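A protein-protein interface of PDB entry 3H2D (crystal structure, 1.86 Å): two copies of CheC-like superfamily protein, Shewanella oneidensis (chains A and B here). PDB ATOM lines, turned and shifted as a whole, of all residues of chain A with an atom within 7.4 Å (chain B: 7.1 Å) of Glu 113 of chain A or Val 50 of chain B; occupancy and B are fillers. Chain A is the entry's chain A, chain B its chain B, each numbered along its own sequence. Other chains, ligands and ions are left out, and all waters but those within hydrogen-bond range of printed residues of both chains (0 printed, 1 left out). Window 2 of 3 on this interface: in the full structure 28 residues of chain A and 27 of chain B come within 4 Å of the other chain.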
ATOM      1  N   ILE A  47     -33.099 -23.891  -7.136  1.00  0.00           N
ATOM      2  CA  ILE A  47     -32.717 -23.080  -5.982  1.00  0.00           C
ATOM      3  C   ILE A  47     -31.443 -23.658  -5.341  1.00  0.00           C
ATOM      4  O   ILE A  47     -31.298 -24.865  -5.205  1.00  0.00           O
ATOM      5  CB  ILE A  47     -33.918 -22.953  -4.984  1.00  0.00           C
ATOM      6  CG1 ILE A  47     -33.684 -21.887  -3.911  1.00  0.00           C
ATOM      7  CG2 ILE A  47     -34.320 -24.318  -4.391  1.00  0.00           C
ATOM      8  CD1 ILE A  47     -34.984 -21.505  -3.203  1.00  0.00           C
ATOM      9  N   GLY A  48     -30.555 -22.773  -4.904  1.00  0.00           N
ATOM     10  CA  GLY A  48     -29.356 -23.159  -4.186  1.00  0.00           C
ATOM     11  C   GLY A  48     -29.593 -23.056  -2.692  1.00  0.00           C
ATOM     12  O   GLY A  48     -30.496 -22.348  -2.248  1.00  0.00           O
ATOM     13  N   MET A  49     -28.753 -23.732  -1.935  1.00  0.00           N
ATOM     14  CA  MET A  49     -28.818 -23.643  -0.491  1.00  0.00           C
ATOM     15  C   MET A  49     -27.452 -23.834   0.144  1.00  0.00           C
ATOM     16  O   MET A  49     -26.567 -24.392  -0.467  1.00  0.00           O
ATOM     17  CB  MET A  49     -29.922 -24.587   0.049  1.00  0.00           C
ATOM     18  CG  MET A  49     -29.745 -26.036   0.060  1.00  0.00           C
ATOM     19  SD  MET A  49     -31.630 -26.764  -0.172  1.00  0.00           S
ATOM     20  CE  MET A  49     -31.353 -26.886  -2.062  1.00  0.00           C
ATOM     21  N   VAL A  50     -27.267 -23.266   1.333  1.00  0.00           N
ATOM     22  CA  VAL A  50     -26.018 -23.433   2.091  1.00  0.00           C
ATOM     23  C   VAL A  50     -26.453 -23.931   3.484  1.00  0.00           C
ATOM     24  O   VAL A  50     -27.446 -23.423   4.033  1.00  0.00           O
ATOM     25  CB  VAL A  50     -25.216 -22.105   2.145  1.00  0.00           C
ATOM     26  CG1 VAL A  50     -24.050 -22.215   3.129  1.00  0.00           C
ATOM     27  CG2 VAL A  50     -24.717 -21.750   0.722  1.00  0.00           C
ATOM     28  N   GLY A  51     -25.752 -24.940   3.997  1.00  0.00           N
ATOM     29  CA  GLY A  51     -26.074 -25.599   5.288  1.00  0.00           C
ATOM     30  C   GLY A  51     -24.828 -25.906   6.099  1.00  0.00           C
ATOM     31  O   GLY A  51     -23.755 -25.409   5.753  1.00  0.00           O
ATOM     32  N   PRO A  52     -24.970 -26.691   7.211  1.00  0.00           N
ATOM     33  CA  PRO A  52     -23.874 -27.000   8.122  1.00  0.00           C
ATOM     34  C   PRO A  52     -22.830 -27.805   7.393  1.00  0.00           C
ATOM     35  O   PRO A  52     -23.084 -28.953   6.993  1.00  0.00           O
ATOM     36  CB  PRO A  52     -24.520 -27.870   9.218  1.00  0.00           C
ATOM     37  CG  PRO A  52     -25.829 -28.243   8.715  1.00  0.00           C
ATOM     38  CD  PRO A  52     -26.228 -27.340   7.628  1.00  0.00           C
ATOM     39  N   GLY A  56     -25.521 -27.035  -1.567  1.00  0.00           N
ATOM     40  CA  GLY A  56     -26.154 -27.813  -2.557  1.00  0.00           C
ATOM     41  C   GLY A  56     -27.248 -27.115  -3.309  1.00  0.00           C
ATOM     42  O   GLY A  56     -27.352 -25.878  -3.346  1.00  0.00           O
ATOM     43  N   LYS A 102     -36.826 -26.733   5.023  1.00  0.00           N
ATOM     44  CA  LYS A 102     -36.046 -25.917   5.915  1.00  0.00           C
ATOM     45  C   LYS A 102     -36.581 -26.031   7.324  1.00  0.00           C
ATOM     46  O   LYS A 102     -35.801 -26.154   8.270  1.00  0.00           O
ATOM     47  CB  LYS A 102     -36.021 -24.438   5.501  1.00  0.00           C
ATOM     48  CG  LYS A 102     -35.329 -23.486   6.473  1.00  0.00           C
ATOM     49  CD  LYS A 102     -35.272 -22.087   5.870  1.00  0.00           C
ATOM     50  CE  LYS A 102     -34.887 -21.008   6.829  1.00  0.00           C
ATOM     51  NZ  LYS A 102     -33.475 -21.081   7.206  1.00  0.00           N
ATOM     52  N   TYR A 110     -30.632 -28.795  12.112  1.00  0.00           N
ATOM     53  CA  TYR A 110     -29.749 -28.472  10.980  1.00  0.00           C
ATOM     54  C   TYR A 110     -30.296 -27.240  10.279  1.00  0.00           C
ATOM     55  O   TYR A 110     -31.393 -27.279   9.757  1.00  0.00           O
ATOM     56  CB  TYR A 110     -29.670 -29.668  10.053  1.00  0.00           C
ATOM     57  CG  TYR A 110     -28.889 -30.795  10.713  1.00  0.00           C
ATOM     58  CD1 TYR A 110     -27.521 -30.645  10.970  1.00  0.00           C
ATOM     59  CD2 TYR A 110     -29.505 -31.970  11.125  1.00  0.00           C
ATOM     60  CE1 TYR A 110     -26.790 -31.631  11.561  1.00  0.00           C
ATOM     61  CE2 TYR A 110     -28.755 -32.981  11.744  1.00  0.00           C
ATOM     62  CZ  TYR A 110     -27.415 -32.790  11.963  1.00  0.00           C
ATOM     63  OH  TYR A 110     -26.633 -33.733  12.557  1.00  0.00           O
ATOM     64  N   GLU A 111     -29.496 -26.171  10.288  1.00  0.00           N
ATOM     65  CA  GLU A 111     -29.862 -24.894   9.721  1.00  0.00           C
ATOM     66  C   GLU A 111     -29.452 -24.853   8.229  1.00  0.00           C
ATOM     67  O   GLU A 111     -28.291 -25.048   7.890  1.00  0.00           O
ATOM     68  CB  GLU A 111     -29.160 -23.765  10.482  1.00  0.00           C
ATOM     69  CG  GLU A 111     -29.316 -23.791  12.034  1.00  0.00           C
ATOM     70  CD  GLU A 111     -30.695 -23.342  12.520  1.00  0.00           C
ATOM     71  OE1 GLU A 111     -31.705 -23.647  11.835  1.00  0.00           O
ATOM     72  OE2 GLU A 111     -30.777 -22.692  13.591  1.00  0.00           O
ATOM     73  N   PHE A 112     -30.416 -24.668   7.345  1.00  0.00           N
ATOM     74  CA  PHE A 112     -30.129 -24.483   5.914  1.00  0.00           C
ATOM     75  C   PHE A 112     -30.703 -23.107   5.565  1.00  0.00           C
ATOM     76  O   PHE A 112     -31.754 -22.731   6.080  1.00  0.00           O
ATOM     77  CB  PHE A 112     -30.803 -25.554   5.043  1.00  0.00           C
ATOM     78  CG  PHE A 112     -30.065 -26.862   5.036  1.00  0.00           C
ATOM     79  CD1 PHE A 112     -29.277 -27.240   3.954  1.00  0.00           C
ATOM     80  CD2 PHE A 112     -30.069 -27.662   6.150  1.00  0.00           C
ATOM     81  CE1 PHE A 112     -28.568 -28.437   3.991  1.00  0.00           C
ATOM     82  CE2 PHE A 112     -29.359 -28.839   6.183  1.00  0.00           C
ATOM     83  CZ  PHE A 112     -28.614 -29.223   5.100  1.00  0.00           C
ATOM     84  N   GLU A 113     -29.980 -22.358   4.735  1.00  0.00           N
ATOM     85  CA  GLU A 113     -30.420 -21.066   4.240  1.00  0.00           C
ATOM     86  C   GLU A 113     -30.577 -21.264   2.733  1.00  0.00           C
ATOM     87  O   GLU A 113     -29.671 -21.763   2.071  1.00  0.00           O
ATOM     88  CB  GLU A 113     -29.412 -19.966   4.549  1.00  0.00           C
ATOM     89  CG  GLU A 113     -29.497 -19.413   5.975  1.00  0.00           C
ATOM     90  CD  GLU A 113     -30.805 -18.646   6.227  1.00  0.00           C
ATOM     91  OE1 GLU A 113     -31.166 -17.757   5.413  1.00  0.00           O
ATOM     92  OE2 GLU A 113     -31.484 -18.941   7.237  1.00  0.00           O
ATOM     93  N   MET A 114     -31.737 -20.899   2.202  1.00  0.00           N
ATOM     94  CA  MET A 114     -32.021 -21.067   0.784  1.00  0.00           C
ATOM     95  C   MET A 114     -31.821 -19.750   0.044  1.00  0.00           C
ATOM     96  O   MET A 114     -32.134 -18.649   0.553  1.00  0.00           O
ATOM     97  CB  MET A 114     -33.456 -21.588   0.556  1.00  0.00           C
ATOM     98  CG  MET A 114     -33.707 -23.063   0.912  1.00  0.00           C
ATOM     99  SD  MET A 114     -33.134 -23.550   2.707  1.00  0.00           S
ATOM    100  CE  MET A 114     -33.632 -25.457   2.804  1.00  0.00           C
ATOM    101  N   ALA A 115     -31.340 -19.853  -1.184  1.00  0.00           N
ATOM    102  CA  ALA A 115     -31.132 -18.678  -2.023  1.00  0.00           C
ATOM    103  C   ALA A 115     -32.499 -18.356  -2.623  1.00  0.00           C
ATOM    104  O   ALA A 115     -33.508 -18.710  -2.047  1.00  0.00           O
ATOM    105  CB  ALA A 115     -30.050 -18.945  -3.078  1.00  0.00           C
ATOM    106  N   THR A 116     -32.580 -17.644  -3.739  1.00  0.00           N
ATOM    107  CA  THR A 116     -33.884 -17.352  -4.326  1.00  0.00           C
ATOM    108  C   THR A 116     -34.065 -18.201  -5.620  1.00  0.00           C
ATOM    109  O   THR A 116     -33.084 -18.560  -6.263  1.00  0.00           O
ATOM    110  CB  THR A 116     -34.012 -15.858  -4.609  1.00  0.00           C
ATOM    111  OG1 THR A 116     -32.912 -15.456  -5.400  1.00  0.00           O
ATOM    112  CG2 THR A 116     -33.997 -15.030  -3.267  1.00  0.00           C
ATOM    113  N   GLY B  48     -27.154 -20.214  -6.727  1.00  0.00           N
ATOM    114  CA  GLY B  48     -27.660 -19.362  -5.645  1.00  0.00           C
ATOM    115  C   GLY B  48     -26.552 -18.807  -4.787  1.00  0.00           C
ATOM    116  O   GLY B  48     -25.455 -19.384  -4.705  1.00  0.00           O
ATOM    117  N   MET B  49     -26.866 -17.686  -4.118  1.00  0.00           N
ATOM    118  CA  MET B  49     -25.963 -16.994  -3.204  1.00  0.00           C
ATOM    119  C   MET B  49     -26.706 -16.624  -1.941  1.00  0.00           C
ATOM    120  O   MET B  49     -27.850 -16.218  -2.004  1.00  0.00           O
ATOM    121  CB  MET B  49     -25.430 -15.729  -3.842  1.00  0.00           C
ATOM    122  CG  MET B  49     -24.502 -16.011  -5.006  1.00  0.00           C
ATOM    123  SD  MET B  49     -24.138 -14.399  -6.043  1.00  0.00           S
ATOM    124  CE  MET B  49     -25.870 -14.269  -6.964  1.00  0.00           C
ATOM    125  N   VAL B  50     -26.057 -16.814  -0.800  1.00  0.00           N
ATOM    126  CA  VAL B  50     -26.674 -16.513   0.479  1.00  0.00           C
ATOM    127  C   VAL B  50     -25.647 -15.777   1.326  1.00  0.00           C
ATOM    128  O   VAL B  50     -24.505 -16.244   1.482  1.00  0.00           O
ATOM    129  CB  VAL B  50     -27.158 -17.776   1.196  1.00  0.00           C
ATOM    130  CG1 VAL B  50     -27.726 -17.458   2.522  1.00  0.00           C
ATOM    131  CG2 VAL B  50     -28.240 -18.508   0.370  1.00  0.00           C
ATOM    132  N   GLY B  51     -26.064 -14.648   1.871  1.00  0.00           N
ATOM    133  CA  GLY B  51     -25.215 -13.847   2.752  1.00  0.00           C
ATOM    134  C   GLY B  51     -25.954 -13.446   4.012  1.00  0.00           C
ATOM    135  O   GLY B  51     -27.136 -13.725   4.138  1.00  0.00           O
ATOM    136  N   PRO B  52     -25.254 -12.800   4.958  1.00  0.00           N
ATOM    137  CA  PRO B  52     -25.875 -12.394   6.211  1.00  0.00           C
ATOM    138  C   PRO B  52     -27.106 -11.526   6.020  1.00  0.00           C
ATOM    139  O   PRO B  52     -28.119 -11.749   6.663  1.00  0.00           O
ATOM    140  CB  PRO B  52     -24.784 -11.575   6.904  1.00  0.00           C
ATOM    141  CG  PRO B  52     -23.524 -12.012   6.311  1.00  0.00           C
ATOM    142  CD  PRO B  52     -23.828 -12.426   4.912  1.00  0.00           C
ATOM    143  N   GLN B  53     -27.015 -10.557   5.122  1.00  0.00           N
ATOM    144  CA  GLN B  53     -28.107  -9.648   4.886  1.00  0.00           C
ATOM    145  C   GLN B  53     -28.496  -9.734   3.405  1.00  0.00           C
ATOM    146  O   GLN B  53     -28.857  -8.734   2.786  1.00  0.00           O
ATOM    147  CB  GLN B  53     -27.681  -8.219   5.268  1.00  0.00           C
ATOM    148  N   THR B  54     -28.452 -10.935   2.828  1.00  0.00           N
ATOM    149  CA  THR B  54     -28.717 -11.037   1.407  1.00  0.00           C
ATOM    150  C   THR B  54     -29.004 -12.447   0.908  1.00  0.00           C
ATOM    151  O   THR B  54     -28.525 -13.435   1.456  1.00  0.00           O
ATOM    152  CB  THR B  54     -27.572 -10.386   0.579  1.00  0.00           C
ATOM    153  OG1 THR B  54     -28.114  -9.907  -0.663  1.00  0.00           O
ATOM    154  CG2 THR B  54     -26.384 -11.356   0.310  1.00  0.00           C
ATOM    155  N   LYS B  55     -29.852 -12.525  -0.107  1.00  0.00           N
ATOM    156  CA  LYS B  55     -29.924 -13.735  -0.898  1.00  0.00           C
ATOM    157  C   LYS B  55     -30.206 -13.420  -2.363  1.00  0.00           C
ATOM    158  O   LYS B  55     -30.851 -12.438  -2.701  1.00  0.00           O
ATOM    159  CB  LYS B  55     -30.900 -14.750  -0.328  1.00  0.00           C
ATOM    160  CG  LYS B  55     -32.338 -14.379  -0.256  1.00  0.00           C
ATOM    161  CD  LYS B  55     -33.198 -15.511   0.344  1.00  0.00           C
ATOM    162  CE  LYS B  55     -32.765 -15.884   1.757  1.00  0.00           C
ATOM    163  NZ  LYS B  55     -33.706 -16.862   2.341  1.00  0.00           N
ATOM    164  N   GLY B  56     -29.709 -14.270  -3.241  1.00  0.00           N
ATOM    165  CA  GLY B  56     -29.979 -14.042  -4.631  1.00  0.00           C
ATOM    166  C   GLY B  56     -29.542 -15.133  -5.533  1.00  0.00           C
ATOM    167  O   GLY B  56     -29.234 -16.232  -5.094  1.00  0.00           O
ATOM    168  N   GLU B 111     -20.769  -9.482   1.773  1.00  0.00           N
ATOM    169  CA  GLU B 111     -20.498 -10.899   2.009  1.00  0.00           C
ATOM    170  C   GLU B 111     -21.616 -11.839   1.522  1.00  0.00           C
ATOM    171  O   GLU B 111     -22.799 -11.670   1.843  1.00  0.00           O
ATOM    172  CB  GLU B 111     -20.284 -11.138   3.477  1.00  0.00           C
ATOM    173  CG  GLU B 111     -19.037 -10.410   4.018  1.00  0.00           C
ATOM    174  N   PHE B 112     -21.202 -12.869   0.804  1.00  0.00           N
ATOM    175  CA  PHE B 112     -22.108 -13.987   0.478  1.00  0.00           C
ATOM    176  C   PHE B 112     -21.296 -15.234   0.265  1.00  0.00           C
ATOM    177  O   PHE B 112     -20.066 -15.186   0.028  1.00  0.00           O
ATOM    178  CB  PHE B 112     -23.001 -13.716  -0.750  1.00  0.00           C
ATOM    179  CG  PHE B 112     -22.273 -13.672  -2.046  1.00  0.00           C
ATOM    180  CD1 PHE B 112     -22.064 -14.812  -2.801  1.00  0.00           C
ATOM    181  CD2 PHE B 112     -21.830 -12.454  -2.541  1.00  0.00           C
ATOM    182  CE1 PHE B 112     -21.373 -14.742  -4.031  1.00  0.00           C
ATOM    183  CE2 PHE B 112     -21.165 -12.373  -3.721  1.00  0.00           C
ATOM    184  CZ  PHE B 112     -20.933 -13.493  -4.488  1.00  0.00           C
ATOM    185  N   GLU B 113     -22.008 -16.364   0.375  1.00  0.00           N
ATOM    186  CA  GLU B 113     -21.492 -17.694   0.076  1.00  0.00           C
ATOM    187  C   GLU B 113     -22.315 -18.204  -1.113  1.00  0.00           C
ATOM    188  O   GLU B 113     -23.525 -17.964  -1.199  1.00  0.00           O
ATOM    189  CB  GLU B 113     -21.708 -18.643   1.258  1.00  0.00           C
ATOM    190  CG  GLU B 113     -20.948 -18.345   2.529  1.00  0.00           C
ATOM    191  CD  GLU B 113     -19.468 -18.240   2.288  1.00  0.00           C
ATOM    192  OE1 GLU B 113     -18.957 -18.980   1.420  1.00  0.00           O
ATOM    193  OE2 GLU B 113     -18.816 -17.403   2.967  1.00  0.00           O
ATOM    194  N   MET B 114     -21.645 -18.877  -2.034  1.00  0.00           N
ATOM    195  CA  MET B 114     -22.297 -19.532  -3.164  1.00  0.00           C
ATOM    196  C   MET B 114     -22.749 -20.940  -2.793  1.00  0.00           C
ATOM    197  O   MET B 114     -22.139 -21.607  -1.956  1.00  0.00           O
ATOM    198  CB  MET B 114     -21.355 -19.612  -4.365  1.00  0.00           C
ATOM    199  CG  MET B 114     -20.243 -20.625  -4.304  1.00  0.00           C
ATOM    200  SD  MET B 114     -19.115 -20.418  -5.939  1.00  0.00           S
ATOM    201  CE  MET B 114     -18.296 -18.864  -5.286  1.00  0.00           C
ATOM    202  N   ALA B 115     -23.809 -21.383  -3.462  1.00  0.00           N
ATOM    203  CA  ALA B 115     -24.267 -22.751  -3.378  1.00  0.00           C
ATOM    204  C   ALA B 115     -23.482 -23.462  -4.483  1.00  0.00           C
ATOM    205  O   ALA B 115     -22.309 -23.169  -4.672  1.00  0.00           O
ATOM    206  CB  ALA B 115     -25.777 -22.815  -3.592  1.00  0.00           C
ATOM    207  N   PHE B 153     -30.906  -9.918  -6.418  1.00  0.00           N
ATOM    208  CA  PHE B 153     -30.696 -10.035  -4.959  1.00  0.00           C
ATOM    209  C   PHE B 153     -31.885  -9.450  -4.247  1.00  0.00           C
ATOM    210  O   PHE B 153     -32.423  -8.440  -4.706  1.00  0.00           O
ATOM    211  CB  PHE B 153     -29.476  -9.257  -4.520  1.00  0.00           C
ATOM    212  CG  PHE B 153     -28.179  -9.913  -4.855  1.00  0.00           C
ATOM    213  CD1 PHE B 153     -27.739 -11.026  -4.136  1.00  0.00           C
ATOM    214  CD2 PHE B 153     -27.375  -9.408  -5.870  1.00  0.00           C
ATOM    215  CE1 PHE B 153     -26.532 -11.636  -4.445  1.00  0.00           C
ATOM    216  CE2 PHE B 153     -26.162 -10.008  -6.178  1.00  0.00           C
ATOM    217  CZ  PHE B 153     -25.746 -11.128  -5.460  1.00  0.00           C
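Of the printed residues of chain A, Val 50 of chain B touches Glu 113, Met 114 and Ala 115.
Of the printed residues of chain A, Met 114 of chain B touches Val 50.
Printed residues of chain A within 4 Å of Gly 56 of chain B: Ala 115 (3.5 Å) and Thr 116 (3.3 Å).
Tyr 110 of chain A touches none of the printed residues of chain B.
The nearest residue of chain B that does not touch Glu 113 of chain A is Lys 55 of chain B (4.1 Å).
The nearest printed residue of chain A that does not touch Val 50 of chain B is Val 50 of chain A (4.7 Å).
Gly 48 of chain A touches Ala 115 of chain B, and with the chains exchanged Ala 115 of chain A touches Gly 48 of chain B.
Val 50 of chain A touches Met 114 of chain B, and with the chains exchanged Met 114 of chain A touches Val 50 of chain B.
Glu 113 of chain A touches Val 50 of chain B, but with the chains exchanged Val 50 of chain A does not touch Glu 113 of chain B (4.4 Å).
Ala 115 of chain A touches Val 50 of chain B, but with the chains exchanged Val 50 of chain A does not touch Ala 115 of chain B (4.2 Å).
Of the 13 pairs that touch across the chains among the printed residues, 8 have their exchanged pair printed and touching as well.
Among the printed residues, merely in contact across the chains: Thr 116 of chain A with Gly 56 of chain B (3.3 Å), Gly 56 of chain A with Ala 115 of chain B (3.5 Å), Ala 115 of chain A with Gly 56 of chain B (3.5 Å), Thr 116 of chain A with Lys 55 of chain B (3.5 Å), Met 49 of chain A with Ala 115 of chain B (3.5 Å), Ala 115 of chain A with Gly 48 of chain B (3.5 Å), Ala 115 of chain A with Met 49 of chain B (3.6 Å), Glu 113 of chain A with Val 50 of chain B (3.6 Å), Gly 48 of chain A with Ala 115 of chain B (3.6 Å), Ala 115 of chain A with Val 50 of chain B (3.7 Å), Val 50 of chain A with Met 114 of chain B (3.7 Å) and Met 114 of chain A with Val 50 of chain B (3.8 Å).
Hydrophobic or aromatic side chains of chain B within 4 Å of the printed part of chain A: Val 50 and Ala 115.
Of the 15 printed residues of chain A, 8 touch a printed residue of chain B.
Printed residues of chain A that touch a printed residue of chain B: Gly 48, Met 49, Val 50, Gly 56, Glu 113, Met 114, Ala 115 and Thr 116.
Hydrophobic or aromatic side chains of chain A within 4 Å of the printed part of chain B: Val 50 and Ala 115.
Among the printed residues, no Asp or Glu carboxylate lies within 4 Å of a Lys or Arg side-chain nitrogen of the other chain.
The backbone carbonyl oxygen of Gly 48 of chain A lies within hydrogen-bond range of the backbone NH of Ala 115 of chain A.
N of Met 49 of chain A lies within hydrogen-bond range of O of Gly 56 of chain A (2.9 Å).
The backbone NH (N) of Glu 113 of chain A sits at hydrogen-bond distance from the backbone carbonyl oxygen (O) of Val 50 of chain A, at 2.8 Å.
The side-chain amino group (NZ) of Lys 102 of chain A lies within salt-bridge range of the side-chain carboxylate (OE2) of Glu 113 of chain A (2.9 Å).
The backbone carbonyl oxygen (O) of Gly 48 of chain B sits at hydrogen-bond distance from the backbone NH (N) of Ala 115 of chain B (2.9 Å).
The backbone NH of Met 49 of chain B lies within hydrogen-bond range of the backbone carbonyl oxygen of Gly 56 of chain B, at 2.9 Å.
O of Met 114 of chain A is in hydrogen-bond range of NZ of Lys 55 of chain B, at 3.0 Å.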
